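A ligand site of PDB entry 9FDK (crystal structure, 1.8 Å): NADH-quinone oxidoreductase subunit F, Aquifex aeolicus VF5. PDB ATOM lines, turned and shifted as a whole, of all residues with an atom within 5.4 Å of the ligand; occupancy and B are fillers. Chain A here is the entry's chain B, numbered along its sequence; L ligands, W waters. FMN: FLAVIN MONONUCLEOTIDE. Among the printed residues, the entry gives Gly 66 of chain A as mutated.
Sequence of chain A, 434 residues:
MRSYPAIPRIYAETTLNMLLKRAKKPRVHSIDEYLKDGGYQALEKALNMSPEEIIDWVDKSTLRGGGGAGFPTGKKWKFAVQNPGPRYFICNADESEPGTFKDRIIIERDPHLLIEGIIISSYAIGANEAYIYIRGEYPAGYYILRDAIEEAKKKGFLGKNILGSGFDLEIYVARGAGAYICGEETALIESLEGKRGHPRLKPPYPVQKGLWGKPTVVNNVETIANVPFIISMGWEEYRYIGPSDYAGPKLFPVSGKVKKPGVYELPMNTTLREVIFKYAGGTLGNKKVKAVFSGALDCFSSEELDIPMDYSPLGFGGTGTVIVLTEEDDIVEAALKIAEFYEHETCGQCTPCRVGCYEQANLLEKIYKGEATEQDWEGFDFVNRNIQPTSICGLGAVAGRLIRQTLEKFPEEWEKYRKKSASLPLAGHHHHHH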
ATOM      1  N   GLY A  65     -26.504 -11.152  25.221  1.00  0.00           N
ATOM      2  CA  GLY A  65     -26.117 -11.962  24.081  1.00  0.00           C
ATOM      3  C   GLY A  65     -26.362 -11.242  22.767  1.00  0.00           C
ATOM      4  O   GLY A  65     -27.359 -10.537  22.621  1.00  0.00           O
ATOM      5  N   GLY A  66     -25.455 -11.423  21.803  1.00  0.00           N
ATOM      6  CA  GLY A  66     -25.613 -10.807  20.494  1.00  0.00           C
ATOM      7  C   GLY A  66     -26.145 -11.770  19.433  1.00  0.00           C
ATOM      8  O   GLY A  66     -26.130 -11.436  18.269  1.00  0.00           O
ATOM      9  N   GLY A  67     -26.587 -12.976  19.833  1.00  0.00           N
ATOM     10  CA  GLY A  67     -27.058 -13.954  18.869  1.00  0.00           C
ATOM     11  C   GLY A  67     -28.574 -13.897  18.631  1.00  0.00           C
ATOM     12  O   GLY A  67     -29.109 -14.750  17.931  1.00  0.00           O
ATOM     13  N   GLY A  68     -29.259 -12.913  19.224  1.00  0.00           N
ATOM     14  CA  GLY A  68     -30.643 -12.637  18.844  1.00  0.00           C
ATOM     15  C   GLY A  68     -31.592 -12.598  20.040  1.00  0.00           C
ATOM     16  O   GLY A  68     -32.593 -11.880  19.995  1.00  0.00           O
ATOM     17  N   ALA A  69     -31.293 -13.369  21.089  1.00  0.00           N
ATOM     18  CA  ALA A  69     -32.199 -13.431  22.229  1.00  0.00           C
ATOM     19  C   ALA A  69     -31.919 -12.376  23.296  1.00  0.00           C
ATOM     20  O   ALA A  69     -32.766 -12.113  24.140  1.00  0.00           O
ATOM     21  CB  ALA A  69     -32.193 -14.843  22.802  1.00  0.00           C
ATOM     22  N   GLY A  70     -30.728 -11.748  23.295  1.00  0.00           N
ATOM     23  CA  GLY A  70     -30.426 -10.690  24.236  1.00  0.00           C
ATOM     24  C   GLY A  70     -30.410 -11.171  25.688  1.00  0.00           C
ATOM     25  O   GLY A  70     -30.677 -10.394  26.615  1.00  0.00           O
ATOM     26  N   PHE A  71     -30.070 -12.448  25.916  1.00  0.00           N
ATOM     27  CA  PHE A  71     -30.060 -12.979  27.269  1.00  0.00           C
ATOM     28  C   PHE A  71     -28.857 -12.432  28.060  1.00  0.00           C
ATOM     29  O   PHE A  71     -27.749 -12.385  27.532  1.00  0.00           O
ATOM     30  CB  PHE A  71     -30.036 -14.512  27.245  1.00  0.00           C
ATOM     31  CG  PHE A  71     -30.414 -15.059  28.615  1.00  0.00           C
ATOM     32  CD1 PHE A  71     -31.746 -15.255  28.962  1.00  0.00           C
ATOM     33  CD2 PHE A  71     -29.436 -15.283  29.574  1.00  0.00           C
ATOM     34  CE1 PHE A  71     -32.087 -15.712  30.230  1.00  0.00           C
ATOM     35  CE2 PHE A  71     -29.779 -15.723  30.844  1.00  0.00           C
ATOM     36  CZ  PHE A  71     -31.100 -15.957  31.167  1.00  0.00           C
ATOM     37  N   THR A  73     -25.572 -12.181  29.906  1.00  0.00           N
ATOM     38  CA  THR A  73     -24.511 -13.160  29.759  1.00  0.00           C
ATOM     39  C   THR A  73     -24.069 -13.685  31.119  1.00  0.00           C
ATOM     40  O   THR A  73     -23.874 -14.898  31.268  1.00  0.00           O
ATOM     41  CB  THR A  73     -23.373 -12.515  28.975  1.00  0.00           C
ATOM     42  OG1 THR A  73     -23.901 -12.113  27.714  1.00  0.00           O
ATOM     43  CG2 THR A  73     -22.208 -13.469  28.790  1.00  0.00           C
ATOM     44  N   LYS A  76     -26.376 -16.225  32.509  1.00  0.00           N
ATOM     45  CA  LYS A  76     -26.171 -17.496  31.816  1.00  0.00           C
ATOM     46  C   LYS A  76     -24.998 -18.265  32.445  1.00  0.00           C
ATOM     47  O   LYS A  76     -25.115 -19.452  32.794  1.00  0.00           O
ATOM     48  CB  LYS A  76     -25.949 -17.314  30.314  1.00  0.00           C
ATOM     49  CG  LYS A  76     -25.955 -18.605  29.492  1.00  0.00           C
ATOM     50  CD  LYS A  76     -25.545 -18.466  28.033  1.00  0.00           C
ATOM     51  CE  LYS A  76     -26.379 -17.517  27.257  1.00  0.00           C
ATOM     52  NZ  LYS A  76     -26.259 -17.711  25.812  1.00  0.00           N
ATOM     53  N   ASN A  92     -20.540 -19.551  19.142  1.00  0.00           N
ATOM     54  CA  ASN A  92     -21.442 -19.705  18.007  1.00  0.00           C
ATOM     55  C   ASN A  92     -21.080 -18.703  16.920  1.00  0.00           C
ATOM     56  O   ASN A  92     -21.395 -17.533  17.033  1.00  0.00           O
ATOM     57  CB  ASN A  92     -22.877 -19.527  18.484  1.00  0.00           C
ATOM     58  CG  ASN A  92     -23.897 -19.941  17.460  1.00  0.00           C
ATOM     59  OD1 ASN A  92     -23.600 -20.008  16.261  1.00  0.00           O
ATOM     60  ND2 ASN A  92     -25.099 -20.234  17.910  1.00  0.00           N
ATOM     61  N   ASP A  94     -22.117 -19.403  13.692  1.00  0.00           N
ATOM     62  CA  ASP A  94     -22.895 -19.963  12.606  1.00  0.00           C
ATOM     63  C   ASP A  94     -23.527 -18.885  11.728  1.00  0.00           C
ATOM     64  O   ASP A  94     -23.972 -19.225  10.633  1.00  0.00           O
ATOM     65  CB  ASP A  94     -23.957 -20.964  13.045  1.00  0.00           C
ATOM     66  CG  ASP A  94     -24.359 -21.889  11.900  1.00  0.00           C
ATOM     67  OD1 ASP A  94     -23.447 -22.617  11.407  1.00  0.00           O
ATOM     68  OD2 ASP A  94     -25.543 -21.794  11.421  1.00  0.00           O
ATOM     69  N   GLU A  95     -23.622 -17.636  12.221  1.00  0.00           N
ATOM     70  CA  GLU A  95     -24.181 -16.473  11.552  1.00  0.00           C
ATOM     71  C   GLU A  95     -24.728 -16.735  10.148  1.00  0.00           C
ATOM     72  O   GLU A  95     -24.006 -16.600   9.163  1.00  0.00           O
ATOM     73  CB  GLU A  95     -23.093 -15.392  11.460  1.00  0.00           C
ATOM     74  CG  GLU A  95     -23.582 -14.120  10.773  1.00  0.00           C
ATOM     75  CD  GLU A  95     -22.653 -12.951  11.053  1.00  0.00           C
ATOM     76  OE1 GLU A  95     -21.547 -12.952  10.470  1.00  0.00           O
ATOM     77  OE2 GLU A  95     -23.047 -12.076  11.863  1.00  0.00           O
ATOM     78  N   SER A  96     -26.017 -17.081  10.034  1.00  0.00           N
ATOM     79  CA  SER A  96     -26.617 -17.382   8.742  1.00  0.00           C
ATOM     80  C   SER A  96     -27.991 -16.739   8.552  1.00  0.00           C
ATOM     81  O   SER A  96     -28.668 -17.038   7.582  1.00  0.00           O
ATOM     82  CB  SER A  96     -26.742 -18.881   8.572  1.00  0.00           C
ATOM     83  OG  SER A  96     -25.473 -19.487   8.449  1.00  0.00           O
ATOM     84  N   GLU A  97     -28.433 -15.880   9.477  1.00  0.00           N
ATOM     85  CA  GLU A  97     -29.692 -15.184   9.282  1.00  0.00           C
ATOM     86  C   GLU A  97     -29.550 -14.138   8.171  1.00  0.00           C
ATOM     87  O   GLU A  97     -28.582 -13.384   8.146  1.00  0.00           O
ATOM     88  CB  GLU A  97     -30.150 -14.457  10.535  1.00  0.00           C
ATOM     89  CG  GLU A  97     -31.578 -13.952  10.339  1.00  0.00           C
ATOM     90  CD  GLU A  97     -32.301 -13.535  11.583  1.00  0.00           C
ATOM     91  OE1 GLU A  97     -31.761 -13.747  12.701  1.00  0.00           O
ATOM     92  OE2 GLU A  97     -33.399 -12.981  11.389  1.00  0.00           O
ATOM     93  N   ASP A 103     -20.743 -10.736  12.662  1.00  0.00           N
ATOM     94  CA  ASP A 103     -19.794 -11.585  13.360  1.00  0.00           C
ATOM     95  C   ASP A 103     -18.560 -11.881  12.515  1.00  0.00           C
ATOM     96  O   ASP A 103     -17.465 -11.978  13.057  1.00  0.00           O
ATOM     97  CB  ASP A 103     -20.417 -12.899  13.796  1.00  0.00           C
ATOM     98  CG  ASP A 103     -21.563 -12.801  14.792  1.00  0.00           C
ATOM     99  OD1 ASP A 103     -21.673 -11.745  15.457  1.00  0.00           O
ATOM    100  OD2 ASP A 103     -22.342 -13.776  14.877  1.00  0.00           O
ATOM    101  N   TYR A 180     -28.905 -23.426   8.407  1.00  0.00           N
ATOM    102  CA  TYR A 180     -29.186 -22.298   9.306  1.00  0.00           C
ATOM    103  C   TYR A 180     -29.536 -22.775  10.707  1.00  0.00           C
ATOM    104  O   TYR A 180     -29.205 -22.121  11.694  1.00  0.00           O
ATOM    105  CB  TYR A 180     -30.316 -21.439   8.748  1.00  0.00           C
ATOM    106  CG  TYR A 180     -30.927 -20.436   9.707  1.00  0.00           C
ATOM    107  CD1 TYR A 180     -30.223 -19.312  10.117  1.00  0.00           C
ATOM    108  CD2 TYR A 180     -32.244 -20.575  10.140  1.00  0.00           C
ATOM    109  CE1 TYR A 180     -30.784 -18.376  10.974  1.00  0.00           C
ATOM    110  CE2 TYR A 180     -32.823 -19.646  10.988  1.00  0.00           C
ATOM    111  CZ  TYR A 180     -32.090 -18.543  11.406  1.00  0.00           C
ATOM    112  OH  TYR A 180     -32.670 -17.642  12.243  1.00  0.00           O
ATOM    113  N   ILE A 181     -30.199 -23.949  10.796  1.00  0.00           N
ATOM    114  CA  ILE A 181     -30.705 -24.417  12.075  1.00  0.00           C
ATOM    115  C   ILE A 181     -29.555 -24.746  13.019  1.00  0.00           C
ATOM    116  O   ILE A 181     -29.756 -24.746  14.221  1.00  0.00           O
ATOM    117  CB  ILE A 181     -31.667 -25.599  11.891  1.00  0.00           C
ATOM    118  CG1 ILE A 181     -32.450 -25.912  13.159  1.00  0.00           C
ATOM    119  CG2 ILE A 181     -30.934 -26.832  11.384  1.00  0.00           C
ATOM    120  CD1 ILE A 181     -33.214 -24.735  13.722  1.00  0.00           C
ATOM    121  N   GLY A 183     -27.359 -22.914  13.924  1.00  0.00           N
ATOM    122  CA  GLY A 183     -27.165 -21.761  14.793  1.00  0.00           C
ATOM    123  C   GLY A 183     -27.942 -21.856  16.106  1.00  0.00           C
ATOM    124  O   GLY A 183     -27.585 -21.199  17.082  1.00  0.00           O
ATOM    125  N   GLU A 184     -29.003 -22.672  16.129  1.00  0.00           N
ATOM    126  CA  GLU A 184     -29.793 -22.897  17.320  1.00  0.00           C
ATOM    127  C   GLU A 184     -28.927 -23.692  18.287  1.00  0.00           C
ATOM    128  O   GLU A 184     -28.335 -24.703  17.882  1.00  0.00           O
ATOM    129  CB  GLU A 184     -31.088 -23.634  16.964  1.00  0.00           C
ATOM    130  CG  GLU A 184     -32.171 -23.502  18.028  1.00  0.00           C
ATOM    131  CD  GLU A 184     -32.144 -24.544  19.135  1.00  0.00           C
ATOM    132  OE1 GLU A 184     -31.394 -25.529  19.042  1.00  0.00           O
ATOM    133  OE2 GLU A 184     -32.935 -24.374  20.096  1.00  0.00           O
ATOM    134  N   GLU A 185     -28.808 -23.234  19.526  1.00  0.00           N
ATOM    135  CA  GLU A 185     -27.736 -23.722  20.403  1.00  0.00           C
ATOM    136  C   GLU A 185     -27.812 -25.243  20.635  1.00  0.00           C
ATOM    137  O   GLU A 185     -26.753 -25.884  20.730  1.00  0.00           O
ATOM    138  CB  GLU A 185     -27.690 -22.946  21.718  1.00  0.00           C
ATOM    139  CG  GLU A 185     -28.969 -23.061  22.543  1.00  0.00           C
ATOM    140  CD  GLU A 185     -28.990 -22.296  23.843  1.00  0.00           C
ATOM    141  OE1 GLU A 185     -27.917 -21.834  24.299  1.00  0.00           O
ATOM    142  OE2 GLU A 185     -30.101 -22.159  24.405  1.00  0.00           O
ATOM    143  N   VAL A 218     -23.120 -21.701  25.490  1.00  0.00           N
ATOM    144  CA  VAL A 218     -23.040 -21.269  24.100  1.00  0.00           C
ATOM    145  C   VAL A 218     -23.197 -19.747  24.116  1.00  0.00           C
ATOM    146  O   VAL A 218     -24.165 -19.238  24.695  1.00  0.00           O
ATOM    147  CB  VAL A 218     -24.125 -21.900  23.211  1.00  0.00           C
ATOM    148  CG1 VAL A 218     -24.035 -21.422  21.770  1.00  0.00           C
ATOM    149  CG2 VAL A 218     -24.110 -23.415  23.282  1.00  0.00           C
ATOM    150  N   ASN A 219     -22.240 -19.056  23.519  1.00  0.00           N
ATOM    151  CA  ASN A 219     -22.360 -17.611  23.331  1.00  0.00           C
ATOM    152  C   ASN A 219     -21.993 -17.240  21.899  1.00  0.00           C
ATOM    153  O   ASN A 219     -21.136 -17.853  21.248  1.00  0.00           O
ATOM    154  CB  ASN A 219     -21.473 -16.806  24.282  1.00  0.00           C
ATOM    155  CG  ASN A 219     -22.144 -16.514  25.604  1.00  0.00           C
ATOM    156  OD1 ASN A 219     -23.234 -15.922  25.686  1.00  0.00           O
ATOM    157  ND2 ASN A 219     -21.478 -16.952  26.653  1.00  0.00           N
ATOM    158  N   ASN A 220     -22.618 -16.156  21.443  1.00  0.00           N
ATOM    159  CA  ASN A 220     -22.372 -15.593  20.134  1.00  0.00           C
ATOM    160  C   ASN A 220     -21.004 -14.896  20.079  1.00  0.00           C
ATOM    161  O   ASN A 220     -20.499 -14.392  21.097  1.00  0.00           O
ATOM    162  CB  ASN A 220     -23.536 -14.656  19.824  1.00  0.00           C
ATOM    163  CG  ASN A 220     -23.346 -13.965  18.515  1.00  0.00           C
ATOM    164  OD1 ASN A 220     -23.537 -14.562  17.440  1.00  0.00           O
ATOM    165  ND2 ASN A 220     -22.956 -12.711  18.593  1.00  0.00           N
ATOM    166  N   VAL A 221     -20.411 -14.877  18.889  1.00  0.00           N
ATOM    167  CA  VAL A 221     -19.143 -14.214  18.599  1.00  0.00           C
ATOM    168  C   VAL A 221     -19.099 -12.812  19.209  1.00  0.00           C
ATOM    169  O   VAL A 221     -18.152 -12.491  19.915  1.00  0.00           O
ATOM    170  CB  VAL A 221     -18.869 -14.154  17.090  1.00  0.00           C
ATOM    171  CG1 VAL A 221     -17.768 -13.141  16.741  1.00  0.00           C
ATOM    172  CG2 VAL A 221     -18.544 -15.530  16.513  1.00  0.00           C
ATOM    173  N   THR A 223     -20.959 -11.379  21.547  1.00  0.00           N
ATOM    174  CA  THR A 223     -20.989 -11.435  23.010  1.00  0.00           C
ATOM    175  C   THR A 223     -19.576 -11.643  23.564  1.00  0.00           C
ATOM    176  O   THR A 223     -19.138 -10.942  24.474  1.00  0.00           O
ATOM    177  CB  THR A 223     -21.917 -12.554  23.485  1.00  0.00           C
ATOM    178  OG1 THR A 223     -23.114 -12.520  22.713  1.00  0.00           O
ATOM    179  CG2 THR A 223     -22.215 -12.439  24.961  1.00  0.00           C
ATOM    180  N   CYS A 393     -38.330 -25.286  18.771  1.00  0.00           N
ATOM    181  CA  CYS A 393     -37.282 -24.285  18.688  1.00  0.00           C
ATOM    182  C   CYS A 393     -37.849 -22.982  18.133  1.00  0.00           C
ATOM    183  O   CYS A 393     -38.977 -22.942  17.675  1.00  0.00           O
ATOM    184  CB  CYS A 393     -36.064 -24.782  17.920  1.00  0.00           C
ATOM    185  SG  CYS A 393     -36.006 -24.380  16.154  1.00  0.00           S
ATOM    186  N   GLY A 394     -37.048 -21.926  18.195  1.00  0.00           N
ATOM    187  CA  GLY A 394     -37.482 -20.586  17.828  1.00  0.00           C
ATOM    188  C   GLY A 394     -37.862 -20.435  16.349  1.00  0.00           C
ATOM    189  O   GLY A 394     -38.616 -19.538  16.018  1.00  0.00           O
ATOM    190  N   LEU A 395     -37.330 -21.283  15.455  1.00  0.00           N
ATOM    191  CA  LEU A 395     -37.587 -21.148  14.036  1.00  0.00           C
ATOM    192  C   LEU A 395     -39.095 -21.279  13.758  1.00  0.00           C
ATOM    193  O   LEU A 395     -39.674 -20.420  13.091  1.00  0.00           O
ATOM    194  CB  LEU A 395     -36.781 -22.145  13.204  1.00  0.00           C
ATOM    195  CG  LEU A 395     -36.788 -21.925  11.690  1.00  0.00           C
ATOM    196  CD1 LEU A 395     -35.546 -22.459  11.036  1.00  0.00           C
ATOM    197  CD2 LEU A 395     -38.027 -22.534  11.024  1.00  0.00           C
HETATM  198  N1  FMN L   1     -27.083 -17.554  17.737  1.00  0.00           N
HETATM  199  C2  FMN L   1     -25.875 -17.190  17.217  1.00  0.00           C
HETATM  200  O2  FMN L   1     -24.926 -16.821  17.979  1.00  0.00           O
HETATM  201  N3  FMN L   1     -25.670 -17.303  15.868  1.00  0.00           N
HETATM  202  C4  FMN L   1     -26.576 -17.826  14.944  1.00  0.00           C
HETATM  203  O4  FMN L   1     -26.258 -17.969  13.768  1.00  0.00           O
HETATM  204  C4A FMN L   1     -27.858 -18.227  15.532  1.00  0.00           C
HETATM  205  N5  FMN L   1     -28.763 -18.781  14.741  1.00  0.00           N
HETATM  206  C5A FMN L   1     -29.949 -19.202  15.329  1.00  0.00           C
HETATM  207  C6  FMN L   1     -30.921 -19.850  14.549  1.00  0.00           C
HETATM  208  C7  FMN L   1     -32.132 -20.246  15.088  1.00  0.00           C
HETATM  209  C7M FMN L   1     -33.159 -20.929  14.192  1.00  0.00           C
HETATM  210  C8  FMN L   1     -32.402 -20.010  16.436  1.00  0.00           C
HETATM  211  C8M FMN L   1     -33.749 -20.310  17.049  1.00  0.00           C
HETATM  212  C9  FMN L   1     -31.440 -19.399  17.232  1.00  0.00           C
HETATM  213  C9A FMN L   1     -30.212 -19.008  16.695  1.00  0.00           C
HETATM  214  N10 FMN L   1     -29.216 -18.405  17.479  1.00  0.00           N
HETATM  215  C10 FMN L   1     -28.016 -18.038  16.922  1.00  0.00           C
HETATM  216  C1' FMN L   1     -29.421 -18.172  18.919  1.00  0.00           C
HETATM  217  C2' FMN L   1     -28.740 -19.263  19.743  1.00  0.00           C
HETATM  218  O2' FMN L   1     -29.622 -20.383  19.902  1.00  0.00           O
HETATM  219  C3' FMN L   1     -28.297 -18.763  21.112  1.00  0.00           C
HETATM  220  O3' FMN L   1     -29.373 -18.058  21.736  1.00  0.00           O
HETATM  221  C4' FMN L   1     -27.015 -17.918  21.121  1.00  0.00           C
HETATM  222  O4' FMN L   1     -25.986 -18.529  20.330  1.00  0.00           O
HETATM  223  C5' FMN L   1     -26.572 -17.679  22.548  1.00  0.00           C
HETATM  224  O5' FMN L   1     -25.452 -16.751  22.621  1.00  0.00           O
HETATM  225  P   FMN L   1     -25.730 -15.296  23.154  1.00  0.00           P
HETATM  226  O1P FMN L   1     -24.293 -14.722  23.286  1.00  0.00           O
HETATM  227  O2P FMN L   1     -26.483 -15.306  24.443  1.00  0.00           O
HETATM  228  O3P FMN L   1     -26.581 -14.590  22.158  1.00  0.00           O
HETATM  229  O   HOH W   1     -30.699 -16.142  13.590  1.00  0.00           O
HETATM  230  O   HOH W   2     -28.992 -15.019  15.085  1.00  0.00           O
HETATM  231  O   HOH W   3     -28.984 -14.661  24.383  1.00  0.00           O
HETATM  232  O   HOH W   4     -32.434 -19.934  20.963  1.00  0.00           O
HETATM  233  O   HOH W   5     -29.089 -15.187  21.552  1.00  0.00           O
HETATM  234  O   HOH W   6     -22.907 -16.446  14.875  1.00  0.00           O
HETATM  235  O   HOH W   7     -31.801 -15.880  17.959  1.00  0.00           O
HETATM  236  O   HOH W   8     -27.413 -19.876  11.902  1.00  0.00           O
HETATM  237  O   HOH W   9     -25.684 -14.047  26.762  1.00  0.00           O
HETATM  238  O   HOH W  10     -27.610 -16.351  12.367  1.00  0.00           O
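The side-chain hydroxyl (OG1) of Thr 223 sits at hydrogen-bond distance from an oxygen (O1P) of the ligand (2.6 Å).
The backbone NH of Asn 220 lies within hydrogen-bond range of an oxygen (O1P) of the ligand (2.9 Å).
O2 of the ligand lies close to OD1 of Asn 220 (2.7 Å).
The side-chain amino group of Lys 76 lies within salt-bridge range of an oxygen (O2P) of the ligand, 2.8 Å away.
N of Gly 67 lies within hydrogen-bond range of O3P of the ligand, 2.8 Å away.
OD1 of Asn 219 lies close to O1P of the ligand (2.9 Å).
The backbone NH of Glu 185 sits at hydrogen-bond distance from an oxygen (O2') of the ligand, at 3.0 Å.
The backbone NH of Glu 95 is in hydrogen-bond range of an oxygen (O4) of the ligand, at 3.1 Å.
The side-chain amide nitrogen (ND2) of Asn 92 is in hydrogen-bond range of an oxygen (O4') of the ligand, 3.1 Å away.
N of Gly 66 is in hydrogen-bond range of O3P of the ligand, 3.4 Å away.
N of Gly 66 is in hydrogen-bond range of OG1 of Thr 223.
OD2 of Asp 103 sits close to OD1 of Asn 220.
The side-chain carboxylate of Glu 95 sits at hydrogen-bond distance from the backbone NH of Asp 103 (2.8 Å).
ND2 of Asn 92 sits at hydrogen-bond distance from O of Gly 183 (2.8 Å).
OD1 of Asn 92 is in hydrogen-bond range of N of Asp 94 (3.0 Å).
O of Asn 92 is in hydrogen-bond range of N of Val 221, 3.4 Å away.
The backbone carbonyl oxygen (O) of Asp 94 sits at hydrogen-bond distance from the side-chain hydroxyl (OG) of Ser 96, at 2.7 Å.
N of Leu 395 sits close to SG of Cys 393 (3.4 Å).
The backbone carbonyl oxygen of Gly 183 lies close to a nitrogen (N10) of the ligand (3.3 Å).
O5' of the ligand sits close to O of Val 218, 3.5 Å away.
Merely in contact with the ligand: Gly 65, Asp 94, Ser 96, Tyr 180, Ile 181, Glu 184, Gly 394 and Leu 395.
Within 4 Å of the ligand: Gly 65, Gly 66, Gly 67, Lys 76, Asn 92, Asp 94, Glu 95, Ser 96, Tyr 180, Ile 181, Gly 183, Glu 184, Glu 185, Val 218, Asn 219, Asn 220, Thr 223, Gly 394 and Leu 395.
Water W10 lies within hydrogen-bond range of an oxygen (O4) of the ligand, the backbone NH (N) of Ser 96 and the backbone NH (N) of Glu 97.
Water W3 bridges an oxygen (O2P) of the ligand (2.6 Å) and the backbone NH of Phe 71 (2.9 Å).
Water W5 lies within hydrogen-bond range of O3P of the ligand (2.6 Å), N of Ala 69 (2.9 Å) and N of Gly 68 (3.3 Å).
Water W9 lies within hydrogen-bond range of an oxygen (O2P) of the ligand (2.8 Å), the backbone carbonyl oxygen of Phe 71 (2.8 Å), the side-chain hydroxyl of Thr 73 (2.8 Å), the side-chain amide oxygen of Asn 219 (3.3 Å) and the backbone NH of Gly 65 (3.4 Å).
Water W1 lies within hydrogen-bond range of OE1 of Glu 97 (2.8 Å), OH of Tyr 180 (2.8 Å) and N5 of the ligand (3.5 Å).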
